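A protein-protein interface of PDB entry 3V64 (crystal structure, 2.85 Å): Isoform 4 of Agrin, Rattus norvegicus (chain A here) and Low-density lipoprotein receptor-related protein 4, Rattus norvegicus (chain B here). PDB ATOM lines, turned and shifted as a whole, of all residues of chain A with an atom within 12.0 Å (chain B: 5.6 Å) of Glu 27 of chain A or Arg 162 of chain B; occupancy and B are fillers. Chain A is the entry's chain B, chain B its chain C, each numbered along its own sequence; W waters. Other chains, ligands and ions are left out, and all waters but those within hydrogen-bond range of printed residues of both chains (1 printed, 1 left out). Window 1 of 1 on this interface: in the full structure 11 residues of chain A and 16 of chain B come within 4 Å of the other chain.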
ATOM      1  N   ALA A  18      16.071 -12.711  -1.048  1.00  0.00           N
ATOM      2  CA  ALA A  18      15.858 -11.508  -0.242  1.00  0.00           C
ATOM      3  C   ALA A  18      16.865 -10.424  -0.618  1.00  0.00           C
ATOM      4  O   ALA A  18      18.078 -10.630  -0.524  1.00  0.00           O
ATOM      5  CB  ALA A  18      15.941 -11.834   1.241  1.00  0.00           C
ATOM      6  N   VAL A  19      16.352  -9.279  -1.060  1.00  0.00           N
ATOM      7  CA  VAL A  19      17.185  -8.205  -1.602  1.00  0.00           C
ATOM      8  C   VAL A  19      17.618  -7.222  -0.513  1.00  0.00           C
ATOM      9  O   VAL A  19      17.138  -7.278   0.623  1.00  0.00           O
ATOM     10  CB  VAL A  19      16.454  -7.442  -2.737  1.00  0.00           C
ATOM     11  CG1 VAL A  19      17.348  -6.381  -3.367  1.00  0.00           C
ATOM     12  CG2 VAL A  19      15.966  -8.405  -3.811  1.00  0.00           C
ATOM     13  N   ILE A  20      18.542  -6.335  -0.876  1.00  0.00           N
ATOM     14  CA  ILE A  20      18.904  -5.199  -0.046  1.00  0.00           C
ATOM     15  C   ILE A  20      17.873  -4.098  -0.263  1.00  0.00           C
ATOM     16  O   ILE A  20      17.609  -3.696  -1.401  1.00  0.00           O
ATOM     17  CB  ILE A  20      20.296  -4.632  -0.408  1.00  0.00           C
ATOM     18  CG1 ILE A  20      21.285  -5.758  -0.753  1.00  0.00           C
ATOM     19  CG2 ILE A  20      20.819  -3.748   0.721  1.00  0.00           C
ATOM     20  CD1 ILE A  20      22.646  -5.269  -1.206  1.00  0.00           C
ATOM     21  N   GLU A  21      17.281  -3.623   0.826  1.00  0.00           N
ATOM     22  CA  GLU A  21      16.447  -2.435   0.759  1.00  0.00           C
ATOM     23  C   GLU A  21      17.292  -1.229   1.148  1.00  0.00           C
ATOM     24  O   GLU A  21      17.468  -0.925   2.330  1.00  0.00           O
ATOM     25  CB  GLU A  21      15.201  -2.574   1.637  1.00  0.00           C
ATOM     26  CG  GLU A  21      15.433  -3.264   2.971  1.00  0.00           C
ATOM     27  CD  GLU A  21      14.144  -3.562   3.713  1.00  0.00           C
ATOM     28  OE1 GLU A  21      14.214  -3.827   4.931  1.00  0.00           O
ATOM     29  OE2 GLU A  21      13.062  -3.531   3.086  1.00  0.00           O
ATOM     30  N   SER A  22      17.824  -0.560   0.130  1.00  0.00           N
ATOM     31  CA  SER A  22      18.718   0.576   0.322  1.00  0.00           C
ATOM     32  C   SER A  22      17.958   1.779   0.860  1.00  0.00           C
ATOM     33  O   SER A  22      18.525   2.632   1.540  1.00  0.00           O
ATOM     34  CB  SER A  22      19.404   0.934  -0.996  1.00  0.00           C
ATOM     35  OG  SER A  22      20.102  -0.182  -1.519  1.00  0.00           O
ATOM     36  N   GLU A  23      16.667   1.831   0.543  1.00  0.00           N
ATOM     37  CA  GLU A  23      15.768   2.866   1.040  1.00  0.00           C
ATOM     38  C   GLU A  23      15.836   2.962   2.564  1.00  0.00           C
ATOM     39  O   GLU A  23      15.970   4.054   3.122  1.00  0.00           O
ATOM     40  CB  GLU A  23      14.328   2.573   0.600  1.00  0.00           C
ATOM     41  CG  GLU A  23      14.105   2.559  -0.910  1.00  0.00           C
ATOM     42  CD  GLU A  23      14.424   1.225  -1.566  1.00  0.00           C
ATOM     43  OE1 GLU A  23      14.810   0.268  -0.857  1.00  0.00           O
ATOM     44  OE2 GLU A  23      14.285   1.129  -2.804  1.00  0.00           O
ATOM     45  N   LEU A  24      15.757   1.808   3.223  1.00  0.00           N
ATOM     46  CA  LEU A  24      15.747   1.737   4.681  1.00  0.00           C
ATOM     47  C   LEU A  24      17.141   1.654   5.296  1.00  0.00           C
ATOM     48  O   LEU A  24      17.381   2.198   6.375  1.00  0.00           O
ATOM     49  CB  LEU A  24      14.906   0.545   5.143  1.00  0.00           C
ATOM     50  CG  LEU A  24      13.394   0.674   4.940  1.00  0.00           C
ATOM     51  CD1 LEU A  24      12.716  -0.686   4.955  1.00  0.00           C
ATOM     52  CD2 LEU A  24      12.791   1.586   5.997  1.00  0.00           C
ATOM     53  N   THR A  25      18.051   0.967   4.611  1.00  0.00           N
ATOM     54  CA  THR A  25      19.374   0.688   5.160  1.00  0.00           C
ATOM     55  C   THR A  25      20.439   1.703   4.755  1.00  0.00           C
ATOM     56  O   THR A  25      21.476   1.801   5.414  1.00  0.00           O
ATOM     57  CB  THR A  25      19.867  -0.716   4.765  1.00  0.00           C
ATOM     58  OG1 THR A  25      19.919  -0.823   3.335  1.00  0.00           O
ATOM     59  CG2 THR A  25      18.938  -1.791   5.322  1.00  0.00           C
ATOM     60  N   ASN A  26      20.183   2.444   3.675  1.00  0.00           N
ATOM     61  CA  ASN A  26      21.179   3.348   3.084  1.00  0.00           C
ATOM     62  C   ASN A  26      22.403   2.576   2.578  1.00  0.00           C
ATOM     63  O   ASN A  26      23.441   3.163   2.269  1.00  0.00           O
ATOM     64  CB  ASN A  26      21.589   4.430   4.090  1.00  0.00           C
ATOM     65  CG  ASN A  26      22.424   5.535   3.469  1.00  0.00           C
ATOM     66  OD1 ASN A  26      22.147   5.999   2.361  1.00  0.00           O
ATOM     67  ND2 ASN A  26      23.452   5.967   4.190  1.00  0.00           N
ATOM     68  N   GLU A  27      22.264   1.258   2.483  1.00  0.00           N
ATOM     69  CA  GLU A  27      23.362   0.394   2.075  1.00  0.00           C
ATOM     70  C   GLU A  27      23.393   0.283   0.557  1.00  0.00           C
ATOM     71  O   GLU A  27      22.349   0.126  -0.079  1.00  0.00           O
ATOM     72  CB  GLU A  27      23.203  -0.993   2.702  1.00  0.00           C
ATOM     73  CG  GLU A  27      24.507  -1.747   2.916  1.00  0.00           C
ATOM     74  CD  GLU A  27      25.107  -1.521   4.294  1.00  0.00           C
ATOM     75  OE1 GLU A  27      24.343  -1.293   5.258  1.00  0.00           O
ATOM     76  OE2 GLU A  27      26.348  -1.581   4.417  1.00  0.00           O
ATOM     77  N   ILE A  28      24.594   0.369  -0.013  1.00  0.00           N
ATOM     78  CA  ILE A  28      24.795   0.258  -1.461  1.00  0.00           C
ATOM     79  C   ILE A  28      24.151  -1.018  -2.013  1.00  0.00           C
ATOM     80  O   ILE A  28      24.469  -2.119  -1.554  1.00  0.00           O
ATOM     81  CB  ILE A  28      26.301   0.267  -1.823  1.00  0.00           C
ATOM     82  CG1 ILE A  28      26.980   1.567  -1.365  1.00  0.00           C
ATOM     83  CG2 ILE A  28      26.510   0.024  -3.314  1.00  0.00           C
ATOM     84  CD1 ILE A  28      26.549   2.811  -2.114  1.00  0.00           C
ATOM     85  N   PRO A  29      23.233  -0.873  -2.991  1.00  0.00           N
ATOM     86  CA  PRO A  29      22.585  -2.035  -3.603  1.00  0.00           C
ATOM     87  C   PRO A  29      23.567  -2.877  -4.408  1.00  0.00           C
ATOM     88  O   PRO A  29      24.482  -2.333  -5.035  1.00  0.00           O
ATOM     89  CB  PRO A  29      21.538  -1.410  -4.532  1.00  0.00           C
ATOM     90  CG  PRO A  29      22.053  -0.046  -4.822  1.00  0.00           C
ATOM     91  CD  PRO A  29      22.736   0.394  -3.559  1.00  0.00           C
ATOM     92  N   ALA A  30      23.367  -4.192  -4.380  1.00  0.00           N
ATOM     93  CA  ALA A  30      24.251  -5.144  -5.047  1.00  0.00           C
ATOM     94  C   ALA A  30      23.720  -6.563  -4.896  1.00  0.00           C
ATOM     95  O   ALA A  30      22.907  -6.841  -4.013  1.00  0.00           O
ATOM     96  CB  ALA A  30      25.657  -5.057  -4.467  1.00  0.00           C
ATOM     97  N   GLU A  31      24.181  -7.456  -5.766  1.00  0.00           N
ATOM     98  CA  GLU A  31      23.995  -8.886  -5.550  1.00  0.00           C
ATOM     99  C   GLU A  31      25.286  -9.654  -5.816  1.00  0.00           C
ATOM    100  O   GLU A  31      25.669  -9.896  -6.965  1.00  0.00           O
ATOM    101  CB  GLU A  31      22.804  -9.445  -6.346  1.00  0.00           C
ATOM    102  CG  GLU A  31      22.742  -9.051  -7.814  1.00  0.00           C
ATOM    103  CD  GLU A  31      21.401  -9.370  -8.450  1.00  0.00           C
ATOM    104  OE1 GLU A  31      20.610 -10.131  -7.849  1.00  0.00           O
ATOM    105  OE2 GLU A  31      21.136  -8.857  -9.556  1.00  0.00           O
ATOM    106  N   LYS A  32      25.961 -10.012  -4.727  1.00  0.00           N
ATOM    107  CA  LYS A  32      27.184 -10.798  -4.788  1.00  0.00           C
ATOM    108  C   LYS A  32      26.827 -12.277  -4.840  1.00  0.00           C
ATOM    109  O   LYS A  32      25.732 -12.672  -4.432  1.00  0.00           O
ATOM    110  CB  LYS A  32      28.056 -10.521  -3.559  1.00  0.00           C
ATOM    111  CG  LYS A  32      28.503  -9.075  -3.410  1.00  0.00           C
ATOM    112  CD  LYS A  32      28.929  -8.781  -1.979  1.00  0.00           C
ATOM    113  CE  LYS A  32      29.410  -7.349  -1.818  1.00  0.00           C
ATOM    114  NZ  LYS A  32      30.733  -7.130  -2.462  1.00  0.00           N
ATOM    115  N   SER B 117      33.005  -3.543   0.346  1.00  0.00           N
ATOM    116  CA  SER B 117      32.109  -2.524  -0.187  1.00  0.00           C
ATOM    117  C   SER B 117      32.855  -1.204  -0.416  1.00  0.00           C
ATOM    118  O   SER B 117      32.741  -0.271   0.385  1.00  0.00           O
ATOM    119  CB  SER B 117      30.896  -2.335   0.729  1.00  0.00           C
ATOM    120  OG  SER B 117      30.108  -3.511   0.782  1.00  0.00           O
ATOM    121  N   GLY B 119      32.866   1.933  -1.525  1.00  0.00           N
ATOM    122  CA  GLY B 119      31.815   2.879  -1.886  1.00  0.00           C
ATOM    123  C   GLY B 119      32.252   4.300  -2.180  1.00  0.00           C
ATOM    124  O   GLY B 119      31.417   5.142  -2.511  1.00  0.00           O
ATOM    125  N   GLY B 120      33.550   4.577  -2.067  1.00  0.00           N
ATOM    126  CA  GLY B 120      34.065   5.926  -2.308  1.00  0.00           C
ATOM    127  C   GLY B 120      35.425   5.963  -2.976  1.00  0.00           C
ATOM    128  O   GLY B 120      36.285   5.130  -2.689  1.00  0.00           O
ATOM    129  N   LEU B 121      35.616   6.938  -3.865  1.00  0.00           N
ATOM    130  CA  LEU B 121      36.874   7.107  -4.592  1.00  0.00           C
ATOM    131  C   LEU B 121      37.312   8.560  -4.683  1.00  0.00           C
ATOM    132  O   LEU B 121      36.483   9.460  -4.830  1.00  0.00           O
ATOM    133  CB  LEU B 121      36.774   6.527  -6.006  1.00  0.00           C
ATOM    134  CG  LEU B 121      37.437   5.171  -6.258  1.00  0.00           C
ATOM    135  CD1 LEU B 121      37.292   4.789  -7.723  1.00  0.00           C
ATOM    136  CD2 LEU B 121      38.911   5.211  -5.877  1.00  0.00           C
ATOM    137  N   THR B 133      37.658   4.299   0.038  1.00  0.00           N
ATOM    138  CA  THR B 133      37.045   3.870   1.287  1.00  0.00           C
ATOM    139  C   THR B 133      36.268   2.574   1.091  1.00  0.00           C
ATOM    140  O   THR B 133      35.652   2.366   0.043  1.00  0.00           O
ATOM    141  CB  THR B 133      36.079   4.938   1.841  1.00  0.00           C
ATOM    142  OG1 THR B 133      34.944   5.060   0.973  1.00  0.00           O
ATOM    143  CG2 THR B 133      36.768   6.292   1.965  1.00  0.00           C
ATOM    144  N   SER B 135      33.376   0.484   3.241  1.00  0.00           N
ATOM    145  CA  SER B 135      32.470   0.401   4.386  1.00  0.00           C
ATOM    146  C   SER B 135      32.414  -1.016   4.955  1.00  0.00           C
ATOM    147  O   SER B 135      32.196  -1.201   6.154  1.00  0.00           O
ATOM    148  CB  SER B 135      31.066   0.882   4.007  1.00  0.00           C
ATOM    149  OG  SER B 135      30.425  -0.029   3.124  1.00  0.00           O
ATOM    150  N   LYS B 160      31.672   2.855   8.892  1.00  0.00           N
ATOM    151  CA  LYS B 160      31.143   2.854   7.533  1.00  0.00           C
ATOM    152  C   LYS B 160      31.576   4.105   6.768  1.00  0.00           C
ATOM    153  O   LYS B 160      30.783   5.033   6.592  1.00  0.00           O
ATOM    154  CB  LYS B 160      29.617   2.718   7.545  1.00  0.00           C
ATOM    155  CG  LYS B 160      29.118   1.319   7.869  1.00  0.00           C
ATOM    156  CD  LYS B 160      27.609   1.305   8.044  1.00  0.00           C
ATOM    157  CE  LYS B 160      27.104  -0.078   8.419  1.00  0.00           C
ATOM    158  NZ  LYS B 160      25.697  -0.017   8.920  1.00  0.00           N
ATOM    159  N   PRO B 161      32.844   4.137   6.314  1.00  0.00           N
ATOM    160  CA  PRO B 161      33.292   5.257   5.494  1.00  0.00           C
ATOM    161  C   PRO B 161      32.634   5.171   4.125  1.00  0.00           C
ATOM    162  O   PRO B 161      32.569   4.086   3.544  1.00  0.00           O
ATOM    163  CB  PRO B 161      34.809   5.036   5.368  1.00  0.00           C
ATOM    164  CG  PRO B 161      35.146   3.873   6.246  1.00  0.00           C
ATOM    165  CD  PRO B 161      33.881   3.097   6.425  1.00  0.00           C
ATOM    166  N   ARG B 162      32.127   6.292   3.630  1.00  0.00           N
ATOM    167  CA  ARG B 162      31.505   6.315   2.315  1.00  0.00           C
ATOM    168  C   ARG B 162      32.176   7.361   1.433  1.00  0.00           C
ATOM    169  O   ARG B 162      33.058   7.032   0.639  1.00  0.00           O
ATOM    170  CB  ARG B 162      29.994   6.556   2.434  1.00  0.00           C
ATOM    171  CG  ARG B 162      29.240   6.522   1.114  1.00  0.00           C
ATOM    172  CD  ARG B 162      27.768   6.226   1.332  1.00  0.00           C
ATOM    173  NE  ARG B 162      27.507   4.789   1.363  1.00  0.00           N
ATOM    174  CZ  ARG B 162      26.328   4.244   1.653  1.00  0.00           C
ATOM    175  NH1 ARG B 162      25.289   5.016   1.946  1.00  0.00           N
ATOM    176  NH2 ARG B 162      26.189   2.924   1.653  1.00  0.00           N
ATOM    177  N   ALA B 163      31.772   8.618   1.592  1.00  0.00           N
ATOM    178  CA  ALA B 163      32.307   9.696   0.772  1.00  0.00           C
ATOM    179  C   ALA B 163      33.726  10.039   1.190  1.00  0.00           C
ATOM    180  O   ALA B 163      34.090   9.891   2.354  1.00  0.00           O
ATOM    181  CB  ALA B 163      31.417  10.921   0.856  1.00  0.00           C
ATOM    182  N   ILE B 164      34.519  10.480   0.219  1.00  0.00           N
ATOM    183  CA  ILE B 164      35.886  10.934   0.450  1.00  0.00           C
ATOM    184  C   ILE B 164      36.224  12.043  -0.545  1.00  0.00           C
ATOM    185  O   ILE B 164      35.865  11.962  -1.723  1.00  0.00           O
ATOM    186  CB  ILE B 164      36.907   9.772   0.361  1.00  0.00           C
ATOM    187  CG1 ILE B 164      38.330  10.269   0.654  1.00  0.00           C
ATOM    188  CG2 ILE B 164      36.818   9.062  -0.987  1.00  0.00           C
ATOM    189  CD1 ILE B 164      39.358   9.167   0.825  1.00  0.00           C
ATOM    190  N   THR B 176      33.229  10.877   4.952  1.00  0.00           N
ATOM    191  CA  THR B 176      32.038  10.699   5.770  1.00  0.00           C
ATOM    192  C   THR B 176      31.973   9.276   6.305  1.00  0.00           C
ATOM    193  O   THR B 176      32.298   8.321   5.599  1.00  0.00           O
ATOM    194  CB  THR B 176      30.746  10.972   4.974  1.00  0.00           C
ATOM    195  OG1 THR B 176      30.579   9.975   3.958  1.00  0.00           O
ATOM    196  CG2 THR B 176      30.769  12.357   4.341  1.00  0.00           C
ATOM    197  N   ASP B 177      31.562   9.149   7.562  1.00  0.00           N
ATOM    198  CA  ASP B 177      31.273   7.851   8.147  1.00  0.00           C
ATOM    199  C   ASP B 177      29.812   7.863   8.575  1.00  0.00           C
ATOM    200  O   ASP B 177      29.416   8.649   9.435  1.00  0.00           O
ATOM    201  CB  ASP B 177      32.191   7.566   9.339  1.00  0.00           C
ATOM    202  CG  ASP B 177      32.185   6.100   9.750  1.00  0.00           C
ATOM    203  OD1 ASP B 177      31.118   5.449   9.685  1.00  0.00           O
ATOM    204  OD2 ASP B 177      33.254   5.599  10.160  1.00  0.00           O
ATOM    205  N   TRP B 178      29.014   6.995   7.960  1.00  0.00           N
ATOM    206  CA  TRP B 178      27.581   6.936   8.238  1.00  0.00           C
ATOM    207  C   TRP B 178      27.217   5.799   9.162  1.00  0.00           C
ATOM    208  O   TRP B 178      26.050   5.411   9.255  1.00  0.00           O
ATOM    209  CB  TRP B 178      26.786   6.868   6.933  1.00  0.00           C
ATOM    210  CG  TRP B 178      26.965   5.584   6.167  1.00  0.00           C
ATOM    211  CD1 TRP B 178      28.040   5.215   5.369  1.00  0.00           C
ATOM    212  CD2 TRP B 178      26.033   4.460   6.096  1.00  0.00           C
ATOM    213  NE1 TRP B 178      27.844   3.970   4.831  1.00  0.00           N
ATOM    214  CE2 TRP B 178      26.654   3.462   5.229  1.00  0.00           C
ATOM    215  CE3 TRP B 178      24.785   4.188   6.649  1.00  0.00           C
ATOM    216  CZ2 TRP B 178      26.040   2.253   4.939  1.00  0.00           C
ATOM    217  CZ3 TRP B 178      24.176   2.966   6.351  1.00  0.00           C
ATOM    218  CH2 TRP B 178      24.791   2.023   5.514  1.00  0.00           C
ATOM    219  N   PRO B 205      25.513  10.594   6.374  1.00  0.00           N
ATOM    220  CA  PRO B 205      26.349  11.462   5.551  1.00  0.00           C
ATOM    221  C   PRO B 205      26.826  10.725   4.296  1.00  0.00           C
ATOM    222  O   PRO B 205      27.905  10.129   4.284  1.00  0.00           O
ATOM    223  CB  PRO B 205      27.518  11.813   6.481  1.00  0.00           C
ATOM    224  CG  PRO B 205      27.592  10.677   7.440  1.00  0.00           C
ATOM    225  CD  PRO B 205      26.173  10.239   7.645  1.00  0.00           C
ATOM    226  N   ASN B 206      25.998  10.757   3.257  1.00  0.00           N
ATOM    227  CA  ASN B 206      26.281  10.046   2.016  1.00  0.00           C
ATOM    228  C   ASN B 206      27.313  10.753   1.146  1.00  0.00           C
ATOM    229  O   ASN B 206      28.361  10.188   0.843  1.00  0.00           O
ATOM    230  CB  ASN B 206      24.991   9.802   1.222  1.00  0.00           C
ATOM    231  CG  ASN B 206      24.239   8.559   1.675  1.00  0.00           C
ATOM    232  OD1 ASN B 206      24.692   7.819   2.551  1.00  0.00           O
ATOM    233  ND2 ASN B 206      23.083   8.321   1.068  1.00  0.00           N
ATOM    234  N   PHE B 249      22.640  10.902  -2.535  1.00  0.00           N
ATOM    235  CA  PHE B 249      23.803  10.025  -2.397  1.00  0.00           C
ATOM    236  C   PHE B 249      25.147  10.736  -2.561  1.00  0.00           C
ATOM    237  O   PHE B 249      25.962  10.738  -1.641  1.00  0.00           O
ATOM    238  CB  PHE B 249      23.712   8.819  -3.340  1.00  0.00           C
ATOM    239  CG  PHE B 249      24.903   7.908  -3.257  1.00  0.00           C
ATOM    240  CD1 PHE B 249      25.061   7.047  -2.180  1.00  0.00           C
ATOM    241  CD2 PHE B 249      25.881   7.932  -4.238  1.00  0.00           C
ATOM    242  CE1 PHE B 249      26.166   6.214  -2.094  1.00  0.00           C
ATOM    243  CE2 PHE B 249      26.987   7.102  -4.161  1.00  0.00           C
ATOM    244  CZ  PHE B 249      27.130   6.241  -3.087  1.00  0.00           C
ATOM    245  N   TRP B 263      18.538   8.652  -4.853  1.00  0.00           N
ATOM    246  CA  TRP B 263      18.044   7.296  -5.081  1.00  0.00           C
ATOM    247  C   TRP B 263      16.552   7.212  -5.206  1.00  0.00           C
ATOM    248  O   TRP B 263      16.036   6.344  -5.911  1.00  0.00           O
ATOM    249  CB  TRP B 263      18.512   6.355  -3.984  1.00  0.00           C
ATOM    250  CG  TRP B 263      19.986   6.063  -4.017  1.00  0.00           C
ATOM    251  CD1 TRP B 263      20.898   6.393  -5.011  1.00  0.00           C
ATOM    252  CD2 TRP B 263      20.760   5.336  -3.014  1.00  0.00           C
ATOM    253  NE1 TRP B 263      22.153   5.946  -4.689  1.00  0.00           N
ATOM    254  CE2 TRP B 263      22.136   5.301  -3.501  1.00  0.00           C
ATOM    255  CE3 TRP B 263      20.460   4.735  -1.797  1.00  0.00           C
ATOM    256  CZ2 TRP B 263      23.152   4.683  -2.789  1.00  0.00           C
ATOM    257  CZ3 TRP B 263      21.493   4.118  -1.085  1.00  0.00           C
ATOM    258  CH2 TRP B 263      22.808   4.097  -1.572  1.00  0.00           C
HETATM  259  O   HOH W   1      27.201  -0.120   1.750  1.00  0.00           O
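NH1 of Arg 162 of chain B sits at hydrogen-bond distance from O of Asn 26 of chain A (2.6 Å).
The side-chain amide oxygen of Asn 206 of chain B lies within hydrogen-bond range of the side-chain amide nitrogen of Asn 26 of chain A (2.8 Å).
NH2 of Arg 162 of chain B lies close to N of Ile 28 of chain A (3.4 Å).
The side-chain hydroxyl (OG1) of Thr 133 of chain B sits at hydrogen-bond distance from the backbone carbonyl oxygen (O) of Arg 162 of chain B (2.7 Å).
O of Lys 160 of chain B lies within hydrogen-bond range of N of Trp 178 of chain B (3.0 Å).
The backbone carbonyl oxygen (O) of Thr 176 of chain B lies within hydrogen-bond range of the backbone NH (N) of Arg 162 of chain B.
The side-chain amide oxygen (OD1) of Asn 206 of chain B is in hydrogen-bond range of the guanidinium group (NH1) of Arg 162 of chain B, at 2.9 Å.
The backbone carbonyl oxygen of Glu 21 of chain A lies within hydrogen-bond range of the side-chain hydroxyl of Thr 25 of chain A (2.7 Å).
The backbone carbonyl oxygen of Glu 27 of chain A lies within hydrogen-bond range of the side-chain hydroxyl of Ser 22 of chain A (2.7 Å).
Ser 22 of chain A touches Trp 263 of chain B (CB to CZ3, 3.8 Å).
Thr 25 of chain A touches Trp 178 of chain B.
ND2 of Asn 26 of chain A touches CE3 of Trp 178 of chain B, at 3.3 Å.
Asn 26 of chain A touches Trp 263 of chain B.
Glu 27 of chain A touches Arg 162 of chain B (CA to NH2, 3.8 Å).
Trp 178 of chain B touches Glu 27 of chain A.
Ile 28 of chain A touches Phe 249 of chain B.
Ile 28 of chain A touches Trp 263 of chain B (CD1 to CZ2, 3.9 Å).
Of chain B, only Arg 162 (3.8 Å) and Trp 178 (3.4 Å) come within 4 Å of Glu 27 of chain A.
Of the printed residues of chain A, Arg 162 of chain B touches Asn 26, Glu 27 and Ile 28.
No residue of chain A comes within 4 Å of Gly 119 of chain B.
No residue of chain A comes within 4 Å of Gly 120 of chain B.
No residue of chain A comes within 4 Å of Thr 133 of chain B.
No residue of chain A comes within 4 Å of Ser 135 of chain B.
No residue of chain A comes within 4 Å of Lys 160 of chain B.
No residue of chain A comes within 4 Å of Pro 161 of chain B.
No residue of chain A comes within 4 Å of Ala 163 of chain B.
No residue of chain A comes within 4 Å of Ile 164 of chain B.
No residue of chain A comes within 4 Å of Thr 176 of chain B.
Of the printed residues of chain B, Ser 22 of chain A touches Trp 263.
Printed residues of chain A within 4 Å of Trp 263 of chain B: Ser 22 (3.8 Å), Asn 26 (3.98 Å) and Ile 28 (3.9 Å).
Of the printed residues of chain B, Asn 26 of chain A touches Arg 162, Trp 178, Asn 206 and Trp 263.
The nearest residue of chain A that does not touch Arg 162 of chain B is Thr 25 of chain A (6.1 Å).
The nearest printed residue of chain B that does not touch Ser 22 of chain A is Arg 162 of chain B (7.2 Å).
Printed residues of chain A that touch a printed residue of chain B: Ser 22, Thr 25, Asn 26, Glu 27 and Ile 28.
Printed residues of chain B that touch a printed residue of chain A: Arg 162, Trp 178, Asn 206, Phe 249 and Trp 263.
Hydrophobic or aromatic side chains of chain B that line the printed part of chain A: Trp 178, Phe 249 and Trp 263.
Water W1 lies within hydrogen-bond range of the side-chain carboxylate of Glu 27 of chain A (3.2 Å), the backbone NH of Ile 28 of chain A (3.2 Å) and the guanidinium group of Arg 162 of chain B (3.2 Å).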
